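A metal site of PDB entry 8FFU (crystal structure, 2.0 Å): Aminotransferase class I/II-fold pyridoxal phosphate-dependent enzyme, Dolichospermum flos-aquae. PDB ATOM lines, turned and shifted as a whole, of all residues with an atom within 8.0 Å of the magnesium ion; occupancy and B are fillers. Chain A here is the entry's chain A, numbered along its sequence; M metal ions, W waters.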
ATOM      1  N   ARG A  62     -18.942  19.564  19.293  1.00  0.00           N
ATOM      2  CA  ARG A  62     -19.376  20.367  18.149  1.00  0.00           C
ATOM      3  C   ARG A  62     -20.768  19.977  17.672  1.00  0.00           C
ATOM      4  O   ARG A  62     -21.513  20.830  17.180  1.00  0.00           O
ATOM      5  CB  ARG A  62     -18.348  20.237  17.028  1.00  0.00           C
ATOM      6  CG  ARG A  62     -17.050  21.003  17.309  1.00  0.00           C
ATOM      7  CD  ARG A  62     -15.964  20.665  16.304  1.00  0.00           C
ATOM      8  NE  ARG A  62     -16.510  20.063  15.095  1.00  0.00           N
ATOM      9  CZ  ARG A  62     -16.203  18.852  14.646  1.00  0.00           C
ATOM     10  NH1 ARG A  62     -15.345  18.070  15.293  1.00  0.00           N
ATOM     11  NH2 ARG A  62     -16.782  18.405  13.538  1.00  0.00           N
ATOM     12  N   GLU A  63     -21.148  18.703  17.817  1.00  0.00           N
ATOM     13  CA  GLU A  63     -22.509  18.282  17.480  1.00  0.00           C
ATOM     14  C   GLU A  63     -23.519  18.812  18.484  1.00  0.00           C
ATOM     15  O   GLU A  63     -24.606  19.260  18.100  1.00  0.00           O
ATOM     16  CB  GLU A  63     -22.591  16.764  17.407  1.00  0.00           C
ATOM     17  CG  GLU A  63     -21.825  16.133  16.240  1.00  0.00           C
ATOM     18  CD  GLU A  63     -22.693  15.913  15.018  1.00  0.00           C
ATOM     19  OE1 GLU A  63     -23.713  16.628  14.862  1.00  0.00           O
ATOM     20  OE2 GLU A  63     -22.357  15.027  14.198  1.00  0.00           O
ATOM     21  N   ALA A  64     -23.186  18.786  19.774  1.00  0.00           N
ATOM     22  CA  ALA A  64     -24.077  19.321  20.797  1.00  0.00           C
ATOM     23  C   ALA A  64     -24.288  20.815  20.624  1.00  0.00           C
ATOM     24  O   ALA A  64     -25.385  21.330  20.857  1.00  0.00           O
ATOM     25  CB  ALA A  64     -23.534  19.003  22.192  1.00  0.00           C
ATOM     26  N   ILE A  65     -23.234  21.541  20.237  1.00  0.00           N
ATOM     27  CA  ILE A  65     -23.369  22.960  19.948  1.00  0.00           C
ATOM     28  C   ILE A  65     -24.207  23.159  18.685  1.00  0.00           C
ATOM     29  O   ILE A  65     -25.125  23.991  18.645  1.00  0.00           O
ATOM     30  CB  ILE A  65     -21.985  23.613  19.789  1.00  0.00           C
ATOM     31  CG1 ILE A  65     -21.191  23.472  21.085  1.00  0.00           C
ATOM     32  CG2 ILE A  65     -22.122  25.073  19.461  1.00  0.00           C
ATOM     33  CD1 ILE A  65     -19.710  23.741  20.907  1.00  0.00           C
ATOM     34  N   ALA A  66     -23.904  22.391  17.632  1.00  0.00           N
ATOM     35  CA  ALA A  66     -24.621  22.543  16.379  1.00  0.00           C
ATOM     36  C   ALA A  66     -26.089  22.164  16.515  1.00  0.00           C
ATOM     37  O   ALA A  66     -26.937  22.719  15.822  1.00  0.00           O
ATOM     38  CB  ALA A  66     -23.958  21.697  15.292  1.00  0.00           C
ATOM     39  N   SER A  67     -26.395  21.216  17.397  1.00  0.00           N
ATOM     40  CA  SER A  67     -27.770  20.775  17.562  1.00  0.00           C
ATOM     41  C   SER A  67     -28.673  21.868  18.118  1.00  0.00           C
ATOM     42  O   SER A  67     -29.896  21.776  17.978  1.00  0.00           O
ATOM     43  CB  SER A  67     -27.840  19.559  18.472  1.00  0.00           C
ATOM     44  OG  SER A  67     -27.622  19.934  19.830  1.00  0.00           O
ATOM     45  N   LEU A  68     -28.107  22.913  18.720  1.00  0.00           N
ATOM     46  CA  LEU A  68     -28.912  23.964  19.329  1.00  0.00           C
ATOM     47  C   LEU A  68     -29.585  24.865  18.296  1.00  0.00           C
ATOM     48  O   LEU A  68     -30.564  25.534  18.637  1.00  0.00           O
ATOM     49  CB  LEU A  68     -28.048  24.819  20.257  1.00  0.00           C
ATOM     50  CG  LEU A  68     -27.312  24.127  21.412  1.00  0.00           C
ATOM     51  CD1 LEU A  68     -26.453  25.129  22.169  1.00  0.00           C
ATOM     52  CD2 LEU A  68     -28.301  23.454  22.350  1.00  0.00           C
ATOM     53  N   ASP A  69     -29.068  24.923  17.077  1.00  0.00           N
ATOM     54  CA  ASP A  69     -29.631  25.808  16.063  1.00  0.00           C
ATOM     55  C   ASP A  69     -29.577  25.113  14.707  1.00  0.00           C
ATOM     56  O   ASP A  69     -28.550  24.532  14.345  1.00  0.00           O
ATOM     57  CB  ASP A  69     -28.852  27.123  15.994  1.00  0.00           C
ATOM     58  CG  ASP A  69     -28.955  27.924  17.277  1.00  0.00           C
ATOM     59  OD1 ASP A  69     -28.269  27.560  18.253  1.00  0.00           O
ATOM     60  OD2 ASP A  69     -29.722  28.907  17.321  1.00  0.00           O
ATOM     61  N   LYS A  70     -30.684  25.199  13.966  1.00  0.00           N
ATOM     62  CA  LYS A  70     -30.722  24.602  12.631  1.00  0.00           C
ATOM     63  C   LYS A  70     -29.758  25.295  11.687  1.00  0.00           C
ATOM     64  O   LYS A  70     -29.274  24.675  10.738  1.00  0.00           O
ATOM     65  CB  LYS A  70     -32.156  24.637  12.085  1.00  0.00           C
ATOM     66  CG  LYS A  70     -32.318  24.167  10.630  1.00  0.00           C
ATOM     67  CD  LYS A  70     -31.662  22.812  10.374  1.00  0.00           C
ATOM     68  CE  LYS A  70     -32.182  21.714  11.297  1.00  0.00           C
ATOM     69  NZ  LYS A  70     -31.216  20.574  11.356  1.00  0.00           N
ATOM     70  N   SER A  71     -29.454  26.565  11.944  1.00  0.00           N
ATOM     71  CA  SER A  71     -28.517  27.292  11.097  1.00  0.00           C
ATOM     72  C   SER A  71     -27.062  26.897  11.326  1.00  0.00           C
ATOM     73  O   SER A  71     -26.185  27.356  10.589  1.00  0.00           O
ATOM     74  CB  SER A  71     -28.690  28.795  11.333  1.00  0.00           C
ATOM     75  OG  SER A  71     -28.444  29.132  12.683  1.00  0.00           O
ATOM     76  N   VAL A  72     -26.769  26.066  12.332  1.00  0.00           N
ATOM     77  CA  VAL A  72     -25.403  25.721  12.711  1.00  0.00           C
ATOM     78  C   VAL A  72     -25.157  24.251  12.411  1.00  0.00           C
ATOM     79  O   VAL A  72     -25.952  23.386  12.791  1.00  0.00           O
ATOM     80  CB  VAL A  72     -25.136  26.027  14.193  1.00  0.00           C
ATOM     81  CG1 VAL A  72     -23.696  25.673  14.547  1.00  0.00           C
ATOM     82  CG2 VAL A  72     -25.405  27.492  14.486  1.00  0.00           C
ATOM     83  N   SER A  73     -24.048  23.976  11.715  1.00  0.00           N
ATOM     84  CA  SER A  73     -23.567  22.638  11.435  1.00  0.00           C
ATOM     85  C   SER A  73     -22.295  22.353  12.234  1.00  0.00           C
ATOM     86  O   SER A  73     -21.574  23.288  12.618  1.00  0.00           O
ATOM     87  CB  SER A  73     -23.298  22.483   9.936  1.00  0.00           C
ATOM     88  OG  SER A  73     -22.419  21.412   9.657  1.00  0.00           O
ATOM     89  N   PRO A  74     -21.992  21.085  12.520  1.00  0.00           N
ATOM     90  CA  PRO A  74     -20.806  20.783  13.356  1.00  0.00           C
ATOM     91  C   PRO A  74     -19.492  21.319  12.807  1.00  0.00           C
ATOM     92  O   PRO A  74     -18.596  21.635  13.603  1.00  0.00           O
ATOM     93  CB  PRO A  74     -20.807  19.253  13.433  1.00  0.00           C
ATOM     94  CG  PRO A  74     -22.226  18.880  13.245  1.00  0.00           C
ATOM     95  CD  PRO A  74     -22.793  19.870  12.274  1.00  0.00           C
ATOM     96  N   ASP A  76     -18.962  24.169  11.428  1.00  0.00           N
ATOM     97  CA  ASP A  76     -18.884  25.625  11.517  1.00  0.00           C
ATOM     98  C   ASP A  76     -18.235  26.095  12.817  1.00  0.00           C
ATOM     99  O   ASP A  76     -18.071  27.300  13.006  1.00  0.00           O
ATOM    100  CB  ASP A  76     -20.277  26.253  11.412  1.00  0.00           C
ATOM    101  CG  ASP A  76     -21.008  25.881  10.144  1.00  0.00           C
ATOM    102  OD1 ASP A  76     -20.396  25.961   9.059  1.00  0.00           O
ATOM    103  OD2 ASP A  76     -22.198  25.512  10.228  1.00  0.00           O
ATOM    104  N   ILE A  77     -17.849  25.177  13.698  1.00  0.00           N
ATOM    105  CA  ILE A  77     -17.543  25.482  15.088  1.00  0.00           C
ATOM    106  C   ILE A  77     -16.063  25.239  15.359  1.00  0.00           C
ATOM    107  O   ILE A  77     -15.494  24.227  14.920  1.00  0.00           O
ATOM    108  CB  ILE A  77     -18.414  24.642  16.032  1.00  0.00           C
ATOM    109  CG1 ILE A  77     -19.891  24.822  15.679  1.00  0.00           C
ATOM    110  CG2 ILE A  77     -18.157  25.001  17.492  1.00  0.00           C
ATOM    111  CD1 ILE A  77     -20.786  23.773  16.256  1.00  0.00           C
HETATM  112 MG    MG M   1     -27.552  22.282  13.687  1.00  0.00          MG
HETATM  113  O   HOH W   1     -28.391  21.664  11.289  1.00  0.00           O
HETATM  114  O   HOH W   2     -27.064  20.351  13.616  1.00  0.00           O
HETATM  115  O   HOH W   3     -30.005  21.891  14.652  1.00  0.00           O
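Of the 15 residues printed, 3 come within 4 Å of the magnesium ion.
The nearest printed residue that does not touch the magnesium ion is Ser 67 (4.03 Å).
The magnesium ion is bound by water W2 (2.0 Å), the backbone carbonyl oxygen (O) of Val 72 (2.1 Å), the backbone carbonyl oxygen (O) of Ala 66 (2.3 Å) and the backbone carbonyl oxygen (O) of Asp 69 (2.5 Å).
The magnesium ion has four donor atoms within binding distance.
Slightly farther from the magnesium ion lies water W1 (2.6 Å).
Slightly farther from the magnesium ion lies water W3 (2.7 Å).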
